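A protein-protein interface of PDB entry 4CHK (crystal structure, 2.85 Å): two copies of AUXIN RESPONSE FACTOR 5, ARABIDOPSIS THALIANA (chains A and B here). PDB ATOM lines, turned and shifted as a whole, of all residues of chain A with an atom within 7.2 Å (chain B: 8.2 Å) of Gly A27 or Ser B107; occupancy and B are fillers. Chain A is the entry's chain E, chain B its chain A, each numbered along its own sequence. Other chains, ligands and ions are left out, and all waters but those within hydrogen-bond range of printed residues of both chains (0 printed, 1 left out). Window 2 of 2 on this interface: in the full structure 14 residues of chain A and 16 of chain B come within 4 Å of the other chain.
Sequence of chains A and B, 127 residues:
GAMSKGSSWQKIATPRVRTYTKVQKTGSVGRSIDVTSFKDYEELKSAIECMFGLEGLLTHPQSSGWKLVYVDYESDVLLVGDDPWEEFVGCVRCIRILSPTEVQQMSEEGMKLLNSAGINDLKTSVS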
ATOM      1  N   LYS A  25     -26.466   6.280   2.594  1.00  0.00           N
ATOM      2  CA  LYS A  25     -25.287   7.008   2.172  1.00  0.00           C
ATOM      3  C   LYS A  25     -24.177   6.605   3.116  1.00  0.00           C
ATOM      4  O   LYS A  25     -24.361   6.610   4.330  1.00  0.00           O
ATOM      5  CB  LYS A  25     -25.511   8.534   2.192  1.00  0.00           C
ATOM      6  CG  LYS A  25     -24.435   9.284   1.413  1.00  0.00           C
ATOM      7  CD  LYS A  25     -24.441  10.777   1.647  1.00  0.00           C
ATOM      8  CE  LYS A  25     -23.030  11.280   1.781  1.00  0.00           C
ATOM      9  NZ  LYS A  25     -22.480  11.048   3.159  1.00  0.00           N
ATOM     10  N   THR A  26     -23.051   6.221   2.557  1.00  0.00           N
ATOM     11  CA  THR A  26     -21.872   5.795   3.274  1.00  0.00           C
ATOM     12  C   THR A  26     -21.317   6.942   4.123  1.00  0.00           C
ATOM     13  O   THR A  26     -20.989   8.006   3.586  1.00  0.00           O
ATOM     14  CB  THR A  26     -20.870   5.243   2.251  1.00  0.00           C
ATOM     15  OG1 THR A  26     -21.462   4.091   1.637  1.00  0.00           O
ATOM     16  CG2 THR A  26     -19.515   4.892   2.870  1.00  0.00           C
ATOM     17  N   GLY A  27     -21.204   6.699   5.432  1.00  0.00           N
ATOM     18  CA  GLY A  27     -20.696   7.682   6.382  1.00  0.00           C
ATOM     19  C   GLY A  27     -21.821   8.545   6.900  1.00  0.00           C
ATOM     20  O   GLY A  27     -21.581   9.500   7.639  1.00  0.00           O
ATOM     21  N   SER A  28     -23.063   8.185   6.545  1.00  0.00           N
ATOM     22  CA  SER A  28     -24.261   8.866   6.990  1.00  0.00           C
ATOM     23  C   SER A  28     -25.245   7.885   7.615  1.00  0.00           C
ATOM     24  O   SER A  28     -25.272   6.709   7.228  1.00  0.00           O
ATOM     25  CB  SER A  28     -24.921   9.590   5.831  1.00  0.00           C
ATOM     26  OG  SER A  28     -24.091  10.665   5.437  1.00  0.00           O
ATOM     27  N   VAL A  29     -26.027   8.369   8.619  1.00  0.00           N
ATOM     28  CA  VAL A  29     -27.094   7.636   9.289  1.00  0.00           C
ATOM     29  C   VAL A  29     -28.159   7.472   8.212  1.00  0.00           C
ATOM     30  O   VAL A  29     -28.501   8.448   7.530  1.00  0.00           O
ATOM     31  CB  VAL A  29     -27.634   8.416  10.529  1.00  0.00           C
ATOM     32  CG1 VAL A  29     -28.975   7.863  11.025  1.00  0.00           C
ATOM     33  CG2 VAL A  29     -26.601   8.444  11.650  1.00  0.00           C
ATOM     34  N   ARG A  96     -29.943   4.135  -2.482  1.00  0.00           N
ATOM     35  CA  ARG A  96     -28.566   4.387  -2.063  1.00  0.00           C
ATOM     36  C   ARG A  96     -27.984   5.549  -2.842  1.00  0.00           C
ATOM     37  O   ARG A  96     -28.069   5.600  -4.063  1.00  0.00           O
ATOM     38  CB  ARG A  96     -27.708   3.143  -2.277  1.00  0.00           C
ATOM     39  CG  ARG A  96     -26.229   3.393  -2.028  1.00  0.00           C
ATOM     40  CD  ARG A  96     -25.542   2.119  -1.663  1.00  0.00           C
ATOM     41  NE  ARG A  96     -25.991   1.626  -0.363  1.00  0.00           N
ATOM     42  CZ  ARG A  96     -25.340   1.879   0.761  1.00  0.00           C
ATOM     43  NH1 ARG A  96     -24.220   2.597   0.741  1.00  0.00           N
ATOM     44  NH2 ARG A  96     -25.802   1.418   1.921  1.00  0.00           N
ATOM     45  N   GLU A 102     -17.179   6.343  -4.786  1.00  0.00           N
ATOM     46  CA  GLU A 102     -17.879   5.044  -4.621  1.00  0.00           C
ATOM     47  C   GLU A 102     -18.185   4.389  -5.973  1.00  0.00           C
ATOM     48  O   GLU A 102     -18.228   3.155  -6.081  1.00  0.00           O
ATOM     49  CB  GLU A 102     -19.234   5.231  -3.900  1.00  0.00           C
ATOM     50  CG  GLU A 102     -19.231   6.028  -2.615  1.00  0.00           C
ATOM     51  CD  GLU A 102     -20.357   5.607  -1.696  1.00  0.00           C
ATOM     52  OE1 GLU A 102     -20.282   4.485  -1.141  1.00  0.00           O
ATOM     53  OE2 GLU A 102     -21.326   6.388  -1.547  1.00  0.00           O
ATOM     54  N   PRO B 100     -23.009  15.412  18.201  1.00  0.00           N
ATOM     55  CA  PRO B 100     -22.580  16.034  16.951  1.00  0.00           C
ATOM     56  C   PRO B 100     -21.165  15.608  16.508  1.00  0.00           C
ATOM     57  O   PRO B 100     -20.922  15.488  15.305  1.00  0.00           O
ATOM     58  CB  PRO B 100     -22.686  17.524  17.271  1.00  0.00           C
ATOM     59  CG  PRO B 100     -23.743  17.615  18.275  1.00  0.00           C
ATOM     60  CD  PRO B 100     -23.559  16.423  19.134  1.00  0.00           C
ATOM     61  N   THR B 101     -20.246  15.337  17.469  1.00  0.00           N
ATOM     62  CA  THR B 101     -18.870  14.902  17.210  1.00  0.00           C
ATOM     63  C   THR B 101     -18.853  13.523  16.603  1.00  0.00           C
ATOM     64  O   THR B 101     -18.085  13.313  15.654  1.00  0.00           O
ATOM     65  CB  THR B 101     -18.040  14.929  18.482  1.00  0.00           C
ATOM     66  OG1 THR B 101     -17.978  16.271  18.966  1.00  0.00           O
ATOM     67  CG2 THR B 101     -16.633  14.431  18.263  1.00  0.00           C
ATOM     68  N   GLU B 102     -19.681  12.561  17.153  1.00  0.00           N
ATOM     69  CA  GLU B 102     -19.728  11.177  16.671  1.00  0.00           C
ATOM     70  C   GLU B 102     -20.266  11.091  15.273  1.00  0.00           C
ATOM     71  O   GLU B 102     -19.787  10.290  14.486  1.00  0.00           O
ATOM     72  CB  GLU B 102     -20.506  10.279  17.607  1.00  0.00           C
ATOM     73  CG  GLU B 102     -19.720   9.823  18.822  1.00  0.00           C
ATOM     74  CD  GLU B 102     -20.540   9.019  19.814  1.00  0.00           C
ATOM     75  OE1 GLU B 102     -21.344   9.624  20.564  1.00  0.00           O
ATOM     76  OE2 GLU B 102     -20.377   7.778  19.834  1.00  0.00           O
ATOM     77  N   VAL B 103     -21.207  11.963  14.932  1.00  0.00           N
ATOM     78  CA  VAL B 103     -21.782  12.066  13.585  1.00  0.00           C
ATOM     79  C   VAL B 103     -20.678  12.437  12.573  1.00  0.00           C
ATOM     80  O   VAL B 103     -20.630  11.829  11.503  1.00  0.00           O
ATOM     81  CB  VAL B 103     -22.923  13.082  13.569  1.00  0.00           C
ATOM     82  CG1 VAL B 103     -23.449  13.263  12.156  1.00  0.00           C
ATOM     83  CG2 VAL B 103     -24.041  12.669  14.545  1.00  0.00           C
ATOM     84  N   GLN B 104     -19.781  13.403  12.913  1.00  0.00           N
ATOM     85  CA  GLN B 104     -18.675  13.748  12.035  1.00  0.00           C
ATOM     86  C   GLN B 104     -17.654  12.619  12.063  1.00  0.00           C
ATOM     87  O   GLN B 104     -17.078  12.300  11.018  1.00  0.00           O
ATOM     88  CB  GLN B 104     -18.054  15.165  12.282  1.00  0.00           C
ATOM     89  CG  GLN B 104     -18.221  15.758  13.681  1.00  0.00           C
ATOM     90  CD  GLN B 104     -17.895  17.238  13.852  1.00  0.00           C
ATOM     91  OE1 GLN B 104     -18.703  18.112  13.483  1.00  0.00           O
ATOM     92  NE2 GLN B 104     -16.766  17.550  14.543  1.00  0.00           N
ATOM     93  N   GLN B 105     -17.468  11.943  13.220  1.00  0.00           N
ATOM     94  CA  GLN B 105     -16.518  10.817  13.252  1.00  0.00           C
ATOM     95  C   GLN B 105     -16.982   9.703  12.345  1.00  0.00           C
ATOM     96  O   GLN B 105     -16.162   9.030  11.792  1.00  0.00           O
ATOM     97  CB  GLN B 105     -16.252  10.281  14.670  1.00  0.00           C
ATOM     98  CG  GLN B 105     -15.278  11.122  15.498  1.00  0.00           C
ATOM     99  CD  GLN B 105     -15.223  10.726  16.960  1.00  0.00           C
ATOM    100  OE1 GLN B 105     -16.005   9.916  17.467  1.00  0.00           O
ATOM    101  NE2 GLN B 105     -14.326  11.342  17.696  1.00  0.00           N
ATOM    102  N   MET B 106     -18.279   9.534  12.169  1.00  0.00           N
ATOM    103  CA  MET B 106     -18.923   8.542  11.311  1.00  0.00           C
ATOM    104  C   MET B 106     -18.660   8.858   9.807  1.00  0.00           C
ATOM    105  O   MET B 106     -18.422   7.950   8.991  1.00  0.00           O
ATOM    106  CB  MET B 106     -20.431   8.571  11.637  1.00  0.00           C
ATOM    107  CG  MET B 106     -21.253   7.623  10.847  1.00  0.00           C
ATOM    108  SD  MET B 106     -22.896   7.289  11.538  1.00  0.00           S
ATOM    109  CE  MET B 106     -23.569   6.462  10.111  1.00  0.00           C
ATOM    110  N   SER B 107     -18.726  10.156   9.461  1.00  0.00           N
ATOM    111  CA  SER B 107     -18.548  10.698   8.118  1.00  0.00           C
ATOM    112  C   SER B 107     -17.145  10.434   7.624  1.00  0.00           C
ATOM    113  O   SER B 107     -16.970   9.927   6.517  1.00  0.00           O
ATOM    114  CB  SER B 107     -18.874  12.190   8.107  1.00  0.00           C
ATOM    115  OG  SER B 107     -18.761  12.718   6.796  1.00  0.00           O
ATOM    116  N   GLU B 108     -16.158  10.733   8.485  1.00  0.00           N
ATOM    117  CA  GLU B 108     -14.720  10.546   8.274  1.00  0.00           C
ATOM    118  C   GLU B 108     -14.360   9.081   8.170  1.00  0.00           C
ATOM    119  O   GLU B 108     -13.481   8.750   7.386  1.00  0.00           O
ATOM    120  CB  GLU B 108     -13.904  11.252   9.370  1.00  0.00           C
ATOM    121  CG  GLU B 108     -13.685  12.735   9.082  1.00  0.00           C
ATOM    122  CD  GLU B 108     -13.678  13.663  10.288  1.00  0.00           C
ATOM    123  OE1 GLU B 108     -12.825  13.462  11.188  1.00  0.00           O
ATOM    124  OE2 GLU B 108     -14.509  14.605  10.321  1.00  0.00           O
ATOM    125  N   GLU B 109     -15.050   8.199   8.910  1.00  0.00           N
ATOM    126  CA  GLU B 109     -14.826   6.759   8.798  1.00  0.00           C
ATOM    127  C   GLU B 109     -15.364   6.164   7.483  1.00  0.00           C
ATOM    128  O   GLU B 109     -14.779   5.201   6.980  1.00  0.00           O
ATOM    129  CB  GLU B 109     -15.218   5.975  10.052  1.00  0.00           C
ATOM    130  CG  GLU B 109     -14.064   5.829  11.048  1.00  0.00           C
ATOM    131  CD  GLU B 109     -14.233   6.474  12.422  1.00  0.00           C
ATOM    132  OE1 GLU B 109     -14.868   5.850  13.312  1.00  0.00           O
ATOM    133  OE2 GLU B 109     -13.687   7.588  12.618  1.00  0.00           O
ATOM    134  N   GLY B 110     -16.384   6.807   6.895  1.00  0.00           N
ATOM    135  CA  GLY B 110     -16.924   6.476   5.578  1.00  0.00           C
ATOM    136  C   GLY B 110     -15.919   6.855   4.506  1.00  0.00           C
ATOM    137  O   GLY B 110     -15.783   6.138   3.512  1.00  0.00           O
ATOM    138  N   MET B 111     -15.153   7.959   4.733  1.00  0.00           N
ATOM    139  CA  MET B 111     -14.072   8.450   3.845  1.00  0.00           C
ATOM    140  C   MET B 111     -12.820   7.558   3.933  1.00  0.00           C
ATOM    141  O   MET B 111     -12.063   7.442   2.975  1.00  0.00           O
ATOM    142  CB  MET B 111     -13.694   9.904   4.184  1.00  0.00           C
ATOM    143  CG  MET B 111     -14.846  10.864   4.052  1.00  0.00           C
ATOM    144  SD  MET B 111     -14.380  12.605   4.117  1.00  0.00           S
ATOM    145  CE  MET B 111     -15.906  13.299   4.831  1.00  0.00           C
ATOM    146  N   LYS B 112     -12.594   6.977   5.115  1.00  0.00           N
ATOM    147  CA  LYS B 112     -11.517   6.046   5.418  1.00  0.00           C
ATOM    148  C   LYS B 112     -11.837   4.730   4.688  1.00  0.00           C
ATOM    149  O   LYS B 112     -10.931   4.138   4.083  1.00  0.00           O
ATOM    150  CB  LYS B 112     -11.423   5.859   6.951  1.00  0.00           C
ATOM    151  CG  LYS B 112     -10.967   4.485   7.422  1.00  0.00           C
ATOM    152  CD  LYS B 112     -10.575   4.516   8.864  1.00  0.00           C
ATOM    153  CE  LYS B 112     -10.894   3.240   9.591  1.00  0.00           C
ATOM    154  NZ  LYS B 112     -12.328   3.172   9.983  1.00  0.00           N
ATOM    155  N   LEU B 113     -13.136   4.292   4.732  1.00  0.00           N
ATOM    156  CA  LEU B 113     -13.626   3.088   4.052  1.00  0.00           C
ATOM    157  C   LEU B 113     -13.409   3.249   2.538  1.00  0.00           C
ATOM    158  O   LEU B 113     -12.805   2.367   1.904  1.00  0.00           O
ATOM    159  CB  LEU B 113     -15.112   2.821   4.359  1.00  0.00           C
ATOM    160  CG  LEU B 113     -15.450   2.091   5.674  1.00  0.00           C
ATOM    161  CD1 LEU B 113     -16.793   2.581   6.258  1.00  0.00           C
ATOM    162  CD2 LEU B 113     -15.490   0.576   5.473  1.00  0.00           C
ATOM    163  N   LEU B 114     -13.829   4.422   1.986  1.00  0.00           N
ATOM    164  CA  LEU B 114     -13.679   4.773   0.563  1.00  0.00           C
ATOM    165  C   LEU B 114     -12.211   5.002   0.095  1.00  0.00           C
ATOM    166  O   LEU B 114     -11.956   4.980  -1.114  1.00  0.00           O
ATOM    167  CB  LEU B 114     -14.599   5.957   0.166  1.00  0.00           C
ATOM    168  CG  LEU B 114     -16.118   5.739   0.279  1.00  0.00           C
ATOM    169  CD1 LEU B 114     -16.858   7.038   0.111  1.00  0.00           C
ATOM    170  CD2 LEU B 114     -16.615   4.699  -0.710  1.00  0.00           C
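The backbone NH of Ser B107 lies close to the backbone carbonyl oxygen of Gly A27 (3.4 Å).
The side-chain amino group (NZ) of Lys A25 is in hydrogen-bond range of the side-chain hydroxyl (OG) of Ser A28.
The side-chain hydroxyl (OG1) of Thr A26 sits at hydrogen-bond distance from the guanidinium group (NH1) of Arg A96, 3.3 Å away.
OG1 of Thr A26 sits at hydrogen-bond distance from OE1 of Glu A102, 3.0 Å away.
Gly B110 touches Thr A26 (O to CG2, 3.99 Å).
CA of Gly A27 touches O of Met B106, 3.5 Å away.
Met B106 touches Ser A28 (CE to C, 3.3 Å).
CE of Met B106 touches N of Val A29, at 3.5 Å.
CG of Glu A102 touches CD2 of Leu B114, at 3.5 Å.
Printed residues of chain B within 4 Å of Thr A26: Gly B110.
Gly A27 touches just these residues of chain B: Met B106 (3.5 Å) and Ser B107 (3.3 Å).
Ser A28 touches one residue of chain B.
Printed residues of chain B within 4 Å of Glu A102: Leu B114.
Ser B107 touches one residue of chain A.
The nearest printed residue of chain B that does not touch Val A29 is Val B103 (5.7 Å).
Of the 15 printed residues of chain B, 4 touch a printed residue of chain A.
Printed residues of chain B that touch a printed residue of chain A: Met B106, Ser B107, Gly B110 and Leu B114.
Hydrophobic or aromatic side chains of chain B that line the printed part of chain A: Met B106 and Leu B114.
Along chain B the printed residues that touch a printed residue of chain A span positions 106 to 114.
Of the 7 printed residues of chain A, 5 touch a printed residue of chain B.
Hydrophobic or aromatic side chains of chain A within 4 Å of the printed part of chain B: Val A29.
Among the printed residues, 6 pairs touch across the chains.
Position printed for both chains: 102.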
